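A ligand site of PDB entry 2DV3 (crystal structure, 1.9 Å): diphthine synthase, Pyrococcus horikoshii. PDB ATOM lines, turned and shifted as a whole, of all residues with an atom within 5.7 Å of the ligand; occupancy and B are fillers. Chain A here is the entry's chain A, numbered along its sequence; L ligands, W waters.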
ATOM      1  N   LEU A  10       8.201 -27.523  -7.595  1.00  0.00           N
ATOM      2  CA  LEU A  10       8.618 -27.787  -6.223  1.00  0.00           C
ATOM      3  C   LEU A  10       9.747 -28.718  -5.847  1.00  0.00           C
ATOM      4  O   LEU A  10      10.554 -28.403  -4.973  1.00  0.00           O
ATOM      5  CB  LEU A  10       7.392 -28.269  -5.450  1.00  0.00           C
ATOM      6  CG  LEU A  10       6.132 -27.419  -5.427  1.00  0.00           C
ATOM      7  CD1 LEU A  10       4.952 -28.288  -5.060  1.00  0.00           C
ATOM      8  CD2 LEU A  10       6.297 -26.284  -4.458  1.00  0.00           C
ATOM      9  N   TYR A  11       9.795 -29.887  -6.483  1.00  0.00           N
ATOM     10  CA  TYR A  11      10.754 -30.890  -6.087  1.00  0.00           C
ATOM     11  C   TYR A  11      11.721 -31.455  -7.126  1.00  0.00           C
ATOM     12  O   TYR A  11      12.927 -31.520  -6.890  1.00  0.00           O
ATOM     13  CB  TYR A  11       9.968 -32.043  -5.443  1.00  0.00           C
ATOM     14  CG  TYR A  11      10.798 -33.120  -4.805  1.00  0.00           C
ATOM     15  CD1 TYR A  11      11.552 -32.857  -3.664  1.00  0.00           C
ATOM     16  CD2 TYR A  11      10.826 -34.408  -5.347  1.00  0.00           C
ATOM     17  CE1 TYR A  11      12.304 -33.852  -3.061  1.00  0.00           C
ATOM     18  CE2 TYR A  11      11.578 -35.417  -4.744  1.00  0.00           C
ATOM     19  CZ  TYR A  11      12.315 -35.124  -3.610  1.00  0.00           C
ATOM     20  OH  TYR A  11      13.060 -36.125  -3.017  1.00  0.00           O
ATOM     21  N   THR A  36      17.104 -19.066  -5.092  1.00  0.00           N
ATOM     22  CA  THR A  36      15.880 -18.620  -4.442  1.00  0.00           C
ATOM     23  C   THR A  36      15.135 -19.746  -3.726  1.00  0.00           C
ATOM     24  O   THR A  36      14.245 -19.500  -2.921  1.00  0.00           O
ATOM     25  CB  THR A  36      14.923 -17.953  -5.447  1.00  0.00           C
ATOM     26  OG1 THR A  36      14.623 -18.872  -6.506  1.00  0.00           O
ATOM     27  CG2 THR A  36      15.555 -16.704  -6.025  1.00  0.00           C
ATOM     28  N   SER A  37      15.504 -20.980  -4.044  1.00  0.00           N
ATOM     29  CA  SER A  37      14.854 -22.120  -3.423  1.00  0.00           C
ATOM     30  C   SER A  37      15.641 -23.398  -3.703  1.00  0.00           C
ATOM     31  O   SER A  37      16.638 -23.389  -4.428  1.00  0.00           O
ATOM     32  CB  SER A  37      13.421 -22.275  -3.944  1.00  0.00           C
ATOM     33  OG  SER A  37      12.739 -23.285  -3.233  1.00  0.00           O
ATOM     34  N   LEU A  38      15.170 -24.503  -3.135  1.00  0.00           N
ATOM     35  CA  LEU A  38      15.840 -25.786  -3.320  1.00  0.00           C
ATOM     36  C   LEU A  38      14.927 -26.857  -3.878  1.00  0.00           C
ATOM     37  O   LEU A  38      13.841 -27.109  -3.348  1.00  0.00           O
ATOM     38  CB  LEU A  38      16.432 -26.269  -1.980  1.00  0.00           C
ATOM     39  CG  LEU A  38      16.900 -27.720  -1.914  1.00  0.00           C
ATOM     40  CD1 LEU A  38      18.050 -27.950  -2.894  1.00  0.00           C
ATOM     41  CD2 LEU A  38      17.337 -28.042  -0.490  1.00  0.00           C
ATOM     42  N   PRO A  85      13.302 -22.323  -9.579  1.00  0.00           N
ATOM     43  CA  PRO A  85      12.561 -23.336  -8.821  1.00  0.00           C
ATOM     44  C   PRO A  85      11.158 -22.779  -8.592  1.00  0.00           C
ATOM     45  O   PRO A  85      10.954 -21.567  -8.674  1.00  0.00           O
ATOM     46  CB  PRO A  85      13.338 -23.421  -7.505  1.00  0.00           C
ATOM     47  CG  PRO A  85      14.721 -22.984  -7.875  1.00  0.00           C
ATOM     48  CD  PRO A  85      14.481 -21.851  -8.839  1.00  0.00           C
ATOM     49  N   GLY A  86      10.194 -23.651  -8.301  1.00  0.00           N
ATOM     50  CA  GLY A  86       8.830 -23.225  -8.055  1.00  0.00           C
ATOM     51  C   GLY A  86       8.272 -22.296  -9.120  1.00  0.00           C
ATOM     52  O   GLY A  86       8.447 -22.535 -10.316  1.00  0.00           O
ATOM     53  N   ASP A  87       7.574 -21.251  -8.684  1.00  0.00           N
ATOM     54  CA  ASP A  87       7.011 -20.258  -9.596  1.00  0.00           C
ATOM     55  C   ASP A  87       8.021 -19.111  -9.589  1.00  0.00           C
ATOM     56  O   ASP A  87       8.385 -18.608  -8.527  1.00  0.00           O
ATOM     57  CB  ASP A  87       5.639 -19.773  -9.131  1.00  0.00           C
ATOM     58  CG  ASP A  87       5.023 -18.755 -10.069  1.00  0.00           C
ATOM     59  OD1 ASP A  87       5.542 -17.623 -10.145  1.00  0.00           O
ATOM     60  OD2 ASP A  87       4.018 -19.090 -10.733  1.00  0.00           O
ATOM     61  N   PRO A  88       8.470 -18.668 -10.765  1.00  0.00           N
ATOM     62  CA  PRO A  88       9.454 -17.591 -10.884  1.00  0.00           C
ATOM     63  C   PRO A  88       9.198 -16.250 -10.189  1.00  0.00           C
ATOM     64  O   PRO A  88      10.143 -15.537  -9.862  1.00  0.00           O
ATOM     65  CB  PRO A  88       9.618 -17.441 -12.400  1.00  0.00           C
ATOM     66  CG  PRO A  88       8.275 -17.800 -12.916  1.00  0.00           C
ATOM     67  CD  PRO A  88       7.920 -19.018 -12.089  1.00  0.00           C
ATOM     68  N   LEU A  89       7.935 -15.917  -9.951  1.00  0.00           N
ATOM     69  CA  LEU A  89       7.638 -14.623  -9.335  1.00  0.00           C
ATOM     70  C   LEU A  89       7.222 -14.635  -7.885  1.00  0.00           C
ATOM     71  O   LEU A  89       7.012 -13.575  -7.293  1.00  0.00           O
ATOM     72  CB  LEU A  89       6.570 -13.905 -10.155  1.00  0.00           C
ATOM     73  CG  LEU A  89       6.853 -13.770 -11.653  1.00  0.00           C
ATOM     74  CD1 LEU A  89       5.732 -12.997 -12.306  1.00  0.00           C
ATOM     75  CD2 LEU A  89       8.189 -13.067 -11.890  1.00  0.00           C
ATOM     76  N   VAL A  90       7.109 -15.822  -7.298  1.00  0.00           N
ATOM     77  CA  VAL A  90       6.685 -15.955  -5.915  1.00  0.00           C
ATOM     78  C   VAL A  90       7.835 -15.912  -4.895  1.00  0.00           C
ATOM     79  O   VAL A  90       8.736 -16.750  -4.919  1.00  0.00           O
ATOM     80  CB  VAL A  90       5.899 -17.279  -5.714  1.00  0.00           C
ATOM     81  CG1 VAL A  90       5.486 -17.433  -4.244  1.00  0.00           C
ATOM     82  CG2 VAL A  90       4.669 -17.273  -6.613  1.00  0.00           C
ATOM     83  N   ALA A  91       7.780 -14.932  -3.995  1.00  0.00           N
ATOM     84  CA  ALA A  91       8.793 -14.788  -2.957  1.00  0.00           C
ATOM     85  C   ALA A  91      10.205 -14.659  -3.539  1.00  0.00           C
ATOM     86  O   ALA A  91      11.165 -15.222  -3.021  1.00  0.00           O
ATOM     87  CB  ALA A  91       8.731 -15.970  -1.988  1.00  0.00           C
ATOM     88  N   THR A  92      10.290 -13.919  -4.637  1.00  0.00           N
ATOM     89  CA  THR A  92      11.557 -13.646  -5.294  1.00  0.00           C
ATOM     90  C   THR A  92      11.392 -12.190  -5.690  1.00  0.00           C
ATOM     91  O   THR A  92      10.337 -11.602  -5.480  1.00  0.00           O
ATOM     92  CB  THR A  92      11.769 -14.469  -6.594  1.00  0.00           C
ATOM     93  OG1 THR A  92      10.864 -14.004  -7.606  1.00  0.00           O
ATOM     94  CG2 THR A  92      11.524 -15.953  -6.334  1.00  0.00           C
ATOM     95  N   PRO A 114       4.102 -25.197 -10.130  1.00  0.00           N
ATOM     96  CA  PRO A 114       3.672 -25.379  -8.739  1.00  0.00           C
ATOM     97  C   PRO A 114       4.554 -24.558  -7.795  1.00  0.00           C
ATOM     98  O   PRO A 114       5.775 -24.541  -7.930  1.00  0.00           O
ATOM     99  CB  PRO A 114       3.850 -26.879  -8.516  1.00  0.00           C
ATOM    100  CG  PRO A 114       3.664 -27.468  -9.874  1.00  0.00           C
ATOM    101  CD  PRO A 114       4.360 -26.488 -10.788  1.00  0.00           C
ATOM    102  N   SER A 115       3.922 -23.884  -6.848  1.00  0.00           N
ATOM    103  CA  SER A 115       4.614 -23.043  -5.872  1.00  0.00           C
ATOM    104  C   SER A 115       4.324 -23.483  -4.449  1.00  0.00           C
ATOM    105  O   SER A 115       3.235 -23.955  -4.144  1.00  0.00           O
ATOM    106  CB  SER A 115       4.171 -21.587  -6.041  1.00  0.00           C
ATOM    107  OG  SER A 115       4.660 -20.794  -4.975  1.00  0.00           O
ATOM    108  N   ILE A 116       5.295 -23.308  -3.561  1.00  0.00           N
ATOM    109  CA  ILE A 116       5.096 -23.690  -2.176  1.00  0.00           C
ATOM    110  C   ILE A 116       3.940 -22.880  -1.589  1.00  0.00           C
ATOM    111  O   ILE A 116       3.239 -23.335  -0.676  1.00  0.00           O
ATOM    112  CB  ILE A 116       6.377 -23.446  -1.343  1.00  0.00           C
ATOM    113  CG1 ILE A 116       6.175 -23.977   0.082  1.00  0.00           C
ATOM    114  CG2 ILE A 116       6.721 -21.953  -1.331  1.00  0.00           C
ATOM    115  CD1 ILE A 116       5.955 -25.485   0.135  1.00  0.00           C
ATOM    116  N   TYR A 117       3.712 -21.697  -2.140  1.00  0.00           N
ATOM    117  CA  TYR A 117       2.648 -20.823  -1.658  1.00  0.00           C
ATOM    118  C   TYR A 117       1.249 -21.460  -1.751  1.00  0.00           C
ATOM    119  O   TYR A 117       0.388 -21.216  -0.905  1.00  0.00           O
ATOM    120  CB  TYR A 117       2.684 -19.468  -2.387  1.00  0.00           C
ATOM    121  CG  TYR A 117       1.839 -18.411  -1.732  1.00  0.00           C
ATOM    122  CD1 TYR A 117       2.212 -17.858  -0.496  1.00  0.00           C
ATOM    123  CD2 TYR A 117       0.647 -17.973  -2.309  1.00  0.00           C
ATOM    124  CE1 TYR A 117       1.408 -16.910   0.139  1.00  0.00           C
ATOM    125  CE2 TYR A 117      -0.161 -17.025  -1.690  1.00  0.00           C
ATOM    126  CZ  TYR A 117       0.236 -16.495  -0.468  1.00  0.00           C
ATOM    127  OH  TYR A 117      -0.557 -15.555   0.163  1.00  0.00           O
ATOM    128  N   LEU A 164       5.465 -19.311   6.915  1.00  0.00           N
ATOM    129  CA  LEU A 164       6.815 -18.847   7.183  1.00  0.00           C
ATOM    130  C   LEU A 164       7.839 -19.486   6.240  1.00  0.00           C
ATOM    131  O   LEU A 164       8.196 -20.660   6.409  1.00  0.00           O
ATOM    132  CB  LEU A 164       7.202 -19.151   8.635  1.00  0.00           C
ATOM    133  CG  LEU A 164       6.382 -18.455   9.735  1.00  0.00           C
ATOM    134  CD1 LEU A 164       6.736 -19.034  11.102  1.00  0.00           C
ATOM    135  CD2 LEU A 164       6.655 -16.972   9.708  1.00  0.00           C
ATOM    136  N   PHE A 165       8.290 -18.708   5.257  1.00  0.00           N
ATOM    137  CA  PHE A 165       9.307 -19.156   4.313  1.00  0.00           C
ATOM    138  C   PHE A 165      10.562 -19.242   5.185  1.00  0.00           C
ATOM    139  O   PHE A 165      10.741 -18.421   6.079  1.00  0.00           O
ATOM    140  CB  PHE A 165       9.532 -18.114   3.209  1.00  0.00           C
ATOM    141  CG  PHE A 165       8.365 -17.942   2.282  1.00  0.00           C
ATOM    142  CD1 PHE A 165       8.112 -18.879   1.270  1.00  0.00           C
ATOM    143  CD2 PHE A 165       7.516 -16.845   2.397  1.00  0.00           C
ATOM    144  CE1 PHE A 165       7.033 -18.720   0.395  1.00  0.00           C
ATOM    145  CE2 PHE A 165       6.437 -16.672   1.523  1.00  0.00           C
ATOM    146  CZ  PHE A 165       6.189 -17.609   0.527  1.00  0.00           C
ATOM    147  N   LEU A 166      11.433 -20.214   4.939  1.00  0.00           N
ATOM    148  CA  LEU A 166      12.646 -20.340   5.738  1.00  0.00           C
ATOM    149  C   LEU A 166      13.876 -19.894   4.944  1.00  0.00           C
ATOM    150  O   LEU A 166      13.929 -20.032   3.727  1.00  0.00           O
ATOM    151  CB  LEU A 166      12.799 -21.781   6.235  1.00  0.00           C
ATOM    152  CG  LEU A 166      11.594 -22.235   7.075  1.00  0.00           C
ATOM    153  CD1 LEU A 166      11.889 -23.586   7.706  1.00  0.00           C
ATOM    154  CD2 LEU A 166      11.274 -21.200   8.145  1.00  0.00           C
ATOM    155  N   ASP A 167      14.863 -19.338   5.647  1.00  0.00           N
ATOM    156  CA  ASP A 167      16.062 -18.812   5.027  1.00  0.00           C
ATOM    157  C   ASP A 167      16.873 -19.817   4.202  1.00  0.00           C
ATOM    158  O   ASP A 167      16.797 -21.030   4.391  1.00  0.00           O
ATOM    159  CB  ASP A 167      16.967 -18.184   6.081  1.00  0.00           C
ATOM    160  CG  ASP A 167      17.738 -16.988   5.551  1.00  0.00           C
ATOM    161  OD1 ASP A 167      17.714 -16.751   4.327  1.00  0.00           O
ATOM    162  OD2 ASP A 167      18.377 -16.293   6.372  1.00  0.00           O
ATOM    163  N   ILE A 168      17.666 -19.277   3.281  1.00  0.00           N
ATOM    164  CA  ILE A 168      18.512 -20.094   2.425  1.00  0.00           C
ATOM    165  C   ILE A 168      19.805 -19.360   2.069  1.00  0.00           C
ATOM    166  O   ILE A 168      19.791 -18.162   1.768  1.00  0.00           O
ATOM    167  CB  ILE A 168      17.764 -20.451   1.117  1.00  0.00           C
ATOM    168  CG1 ILE A 168      18.705 -21.211   0.179  1.00  0.00           C
ATOM    169  CG2 ILE A 168      17.245 -19.197   0.443  1.00  0.00           C
ATOM    170  CD1 ILE A 168      18.044 -21.652  -1.119  1.00  0.00           C
ATOM    171  N   LEU A 206       5.945 -28.612   6.805  1.00  0.00           N
ATOM    172  CA  LEU A 206       5.823 -29.248   5.499  1.00  0.00           C
ATOM    173  C   LEU A 206       7.231 -29.303   4.921  1.00  0.00           C
ATOM    174  O   LEU A 206       7.880 -28.274   4.751  1.00  0.00           O
ATOM    175  CB  LEU A 206       4.892 -28.441   4.573  1.00  0.00           C
ATOM    176  CG  LEU A 206       4.791 -28.916   3.113  1.00  0.00           C
ATOM    177  CD1 LEU A 206       4.428 -30.393   3.064  1.00  0.00           C
ATOM    178  CD2 LEU A 206       3.758 -28.079   2.368  1.00  0.00           C
ATOM    179  N   ALA A 207       7.706 -30.516   4.639  1.00  0.00           N
ATOM    180  CA  ALA A 207       9.039 -30.693   4.100  1.00  0.00           C
ATOM    181  C   ALA A 207       8.996 -31.406   2.763  1.00  0.00           C
ATOM    182  O   ALA A 207       8.314 -32.414   2.601  1.00  0.00           O
ATOM    183  CB  ALA A 207       9.900 -31.474   5.083  1.00  0.00           C
ATOM    184  N   ARG A 208       9.749 -30.870   1.806  1.00  0.00           N
ATOM    185  CA  ARG A 208       9.847 -31.430   0.460  1.00  0.00           C
ATOM    186  C   ARG A 208       8.506 -31.591  -0.239  1.00  0.00           C
ATOM    187  O   ARG A 208       8.187 -32.656  -0.770  1.00  0.00           O
ATOM    188  CB  ARG A 208      10.592 -32.774   0.511  1.00  0.00           C
ATOM    189  CG  ARG A 208      11.932 -32.683   1.227  1.00  0.00           C
ATOM    190  CD  ARG A 208      12.584 -34.055   1.359  1.00  0.00           C
ATOM    191  NE  ARG A 208      11.738 -34.983   2.103  1.00  0.00           N
ATOM    192  CZ  ARG A 208      11.446 -34.877   3.397  1.00  0.00           C
ATOM    193  NH1 ARG A 208      11.943 -33.867   4.109  1.00  0.00           N
ATOM    194  NH2 ARG A 208      10.659 -35.753   3.979  1.00  0.00           N
ATOM    195  N   ALA A 209       7.714 -30.527  -0.238  1.00  0.00           N
ATOM    196  CA  ALA A 209       6.432 -30.558  -0.929  1.00  0.00           C
ATOM    197  C   ALA A 209       6.809 -30.827  -2.384  1.00  0.00           C
ATOM    198  O   ALA A 209       7.892 -30.447  -2.815  1.00  0.00           O
ATOM    199  CB  ALA A 209       5.738 -29.203  -0.814  1.00  0.00           C
ATOM    200  N   GLY A 210       5.923 -31.490  -3.125  1.00  0.00           N
ATOM    201  CA  GLY A 210       6.234 -31.782  -4.512  1.00  0.00           C
ATOM    202  C   GLY A 210       6.704 -33.206  -4.700  1.00  0.00           C
ATOM    203  O   GLY A 210       6.511 -33.800  -5.754  1.00  0.00           O
ATOM    204  N   PRO A 233      13.973 -28.747   1.304  1.00  0.00           N
ATOM    205  CA  PRO A 233      13.514 -27.554   2.003  1.00  0.00           C
ATOM    206  C   PRO A 233      12.348 -27.791   2.962  1.00  0.00           C
ATOM    207  O   PRO A 233      11.577 -28.743   2.820  1.00  0.00           O
ATOM    208  CB  PRO A 233      13.150 -26.612   0.868  1.00  0.00           C
ATOM    209  CG  PRO A 233      12.567 -27.560  -0.143  1.00  0.00           C
ATOM    210  CD  PRO A 233      13.529 -28.743  -0.106  1.00  0.00           C
ATOM    211  N   HIS A 234      12.238 -26.899   3.943  1.00  0.00           N
ATOM    212  CA  HIS A 234      11.177 -26.945   4.946  1.00  0.00           C
ATOM    213  C   HIS A 234      10.428 -25.635   4.962  1.00  0.00           C
ATOM    214  O   HIS A 234      10.972 -24.585   4.636  1.00  0.00           O
ATOM    215  CB  HIS A 234      11.755 -27.114   6.362  1.00  0.00           C
ATOM    216  CG  HIS A 234      12.376 -28.448   6.624  1.00  0.00           C
ATOM    217  ND1 HIS A 234      12.865 -28.803   7.858  1.00  0.00           N
ATOM    218  CD2 HIS A 234      12.596 -29.510   5.812  1.00  0.00           C
ATOM    219  CE1 HIS A 234      13.359 -30.023   7.799  1.00  0.00           C
ATOM    220  NE2 HIS A 234      13.202 -30.479   6.573  1.00  0.00           N
ATOM    221  N   ILE A 235       9.163 -25.698   5.375  1.00  0.00           N
ATOM    222  CA  ILE A 235       8.355 -24.511   5.509  1.00  0.00           C
ATOM    223  C   ILE A 235       7.683 -24.668   6.870  1.00  0.00           C
ATOM    224  O   ILE A 235       7.358 -25.777   7.286  1.00  0.00           O
ATOM    225  CB  ILE A 235       7.296 -24.412   4.374  1.00  0.00           C
ATOM    226  CG1 ILE A 235       6.893 -22.952   4.181  1.00  0.00           C
ATOM    227  CG2 ILE A 235       6.090 -25.259   4.666  1.00  0.00           C
ATOM    228  CD1 ILE A 235       7.975 -22.126   3.565  1.00  0.00           C
HETATM  229  N1  LIG L   1       9.393 -19.001  -5.990  1.00  0.00           N
HETATM  230  C1  LIG L   1       9.424 -20.147  -4.976  1.00  0.00           C
HETATM  231  C2  LIG L   1       9.664 -19.781  -3.541  1.00  0.00           C
HETATM  232  C3  LIG L   1      10.926 -19.006  -3.169  1.00  0.00           C
HETATM  233  S1  LIG L   1      11.046 -18.998  -1.331  1.00  0.00           S
HETATM  234  C4  LIG L   1       8.044 -20.934  -5.125  1.00  0.00           C
HETATM  235  O1  LIG L   1       7.211 -20.545  -5.961  1.00  0.00           O
HETATM  236  O2  LIG L   1       7.891 -21.968  -4.355  1.00  0.00           O
HETATM  237  C5  LIG L   1      11.920 -20.492  -1.068  1.00  0.00           C
HETATM  238  C6  LIG L   1      11.527 -21.073   0.347  1.00  0.00           C
HETATM  239  O3  LIG L   1      10.175 -21.607   0.229  1.00  0.00           O
HETATM  240  C7  LIG L   1      12.384 -22.196   0.832  1.00  0.00           C
HETATM  241  O4  LIG L   1      13.481 -21.691   1.573  1.00  0.00           O
HETATM  242  C8  LIG L   1      11.369 -23.033   1.657  1.00  0.00           C
HETATM  243  O5  LIG L   1      11.213 -22.519   2.978  1.00  0.00           O
HETATM  244  C9  LIG L   1      10.080 -22.973   0.820  1.00  0.00           C
HETATM  245  N2  LIG L   1       9.983 -23.920  -0.155  1.00  0.00           N
HETATM  246  C10 LIG L   1      10.182 -23.935  -1.528  1.00  0.00           C
HETATM  247  N3  LIG L   1       9.967 -25.085  -2.104  1.00  0.00           N
HETATM  248  C11 LIG L   1       9.596 -25.953  -1.032  1.00  0.00           C
HETATM  249  C12 LIG L   1       9.230 -27.344  -1.024  1.00  0.00           C
HETATM  250  N4  LIG L   1       9.198 -28.120  -2.124  1.00  0.00           N
HETATM  251  N5  LIG L   1       8.922 -27.847   0.223  1.00  0.00           N
HETATM  252  C13 LIG L   1       8.950 -27.106   1.360  1.00  0.00           C
HETATM  253  N6  LIG L   1       9.290 -25.777   1.383  1.00  0.00           N
HETATM  254  C14 LIG L   1       9.602 -25.267   0.159  1.00  0.00           C
HETATM  255  O   HOH W   1      12.204 -29.470  -3.037  1.00  0.00           O
HETATM  256  O   HOH W   2      11.900 -19.577  -6.736  1.00  0.00           O
HETATM  257  O   HOH W   3      15.333 -23.222   2.912  1.00  0.00           O
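The side-chain hydroxyl (OG) of Ser 115 sits close to the backbone NH (N) of Tyr 117.
The backbone NH of Leu 89 lies within hydrogen-bond range of the side-chain carboxylate of Asp 87, at 2.9 Å.
O of Pro 88 lies within hydrogen-bond range of OG1 of Thr 92 (2.8 Å).
The backbone NH (N) of Arg 208 is in hydrogen-bond range of the backbone carbonyl oxygen (O) of Pro 233, 3.0 Å away.
N of Ile 235 sits at hydrogen-bond distance from O of Leu 206, at 2.9 Å.
O of Thr 36 sits close to S1 of the ligand (3.6 Å).
C of Gly 86 touches O1 of the ligand (3.8 Å).
Ala 91 touches the ligand.
Thr 92 touches the ligand (CG2 to N1, 3.7 Å).
Phe 165 touches the ligand.
Leu 206 touches the ligand (O to C13, 3.7 Å).
Arg 208 touches the ligand.
Pro 233 touches the ligand (O to C13, 3.4 Å).
Ile 235 touches the ligand.
Hydrophobic or aromatic side chains that line the ligand: Leu 10, Val 90, Ala 91, Ile 116, Phe 165, Leu 166, Ala 209, Pro 233 and Ile 235.
Within 4 Å of the ligand: Leu 10, Thr 36, Ser 37, Gly 86, Asp 87, Val 90, Ala 91, Thr 92, Ser 115, Ile 116, Phe 165, Leu 166, Leu 206, Arg 208, Ala 209, Pro 233, His 234 and Ile 235.
The backbone carbonyl oxygen of Asp 87 lies within hydrogen-bond range of a nitrogen (N1) of the ligand (2.8 Å).
An oxygen (O1) of the ligand is in hydrogen-bond range of the side-chain hydroxyl of Ser 115.
OG of Ser 37 lies close to N3 of the ligand, at 3.5 Å.
N4 of the ligand is in hydrogen-bond range of O of Ala 209.
An oxygen (O5) of the ligand lies within hydrogen-bond range of the backbone NH of Leu 166 (3.0 Å).
O of Leu 10 is in hydrogen-bond range of N4 of the ligand (3.2 Å).
N of Asp 87 sits at hydrogen-bond distance from O1 of the ligand, at 2.8 Å.
N of Ile 116 is in hydrogen-bond range of O2 of the ligand (3.0 Å).
O5 of the ligand lies within hydrogen-bond range of O of His 234.
The backbone NH (N) of Ala 209 is in hydrogen-bond range of a nitrogen (N5) of the ligand (3.0 Å).
The backbone carbonyl oxygen (O) of Val 90 is in hydrogen-bond range of a nitrogen (N1) of the ligand, at 2.6 Å.
The backbone carbonyl oxygen (O) of Leu 166 is in hydrogen-bond range of an oxygen (O4) of the ligand, 2.8 Å away.
Water W2 lies within hydrogen-bond range of a nitrogen (N1) of the ligand (2.7 Å), the side-chain hydroxyl of Thr 36 (2.8 Å) and the backbone carbonyl oxygen of Pro 85 (2.9 Å).
Water W3 bridges an oxygen (O4) of the ligand and the backbone carbonyl oxygen (O) of Asp 167.
Water W1 lies within hydrogen-bond range of O of Leu 10, O of Leu 38 and N4 of the ligand.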
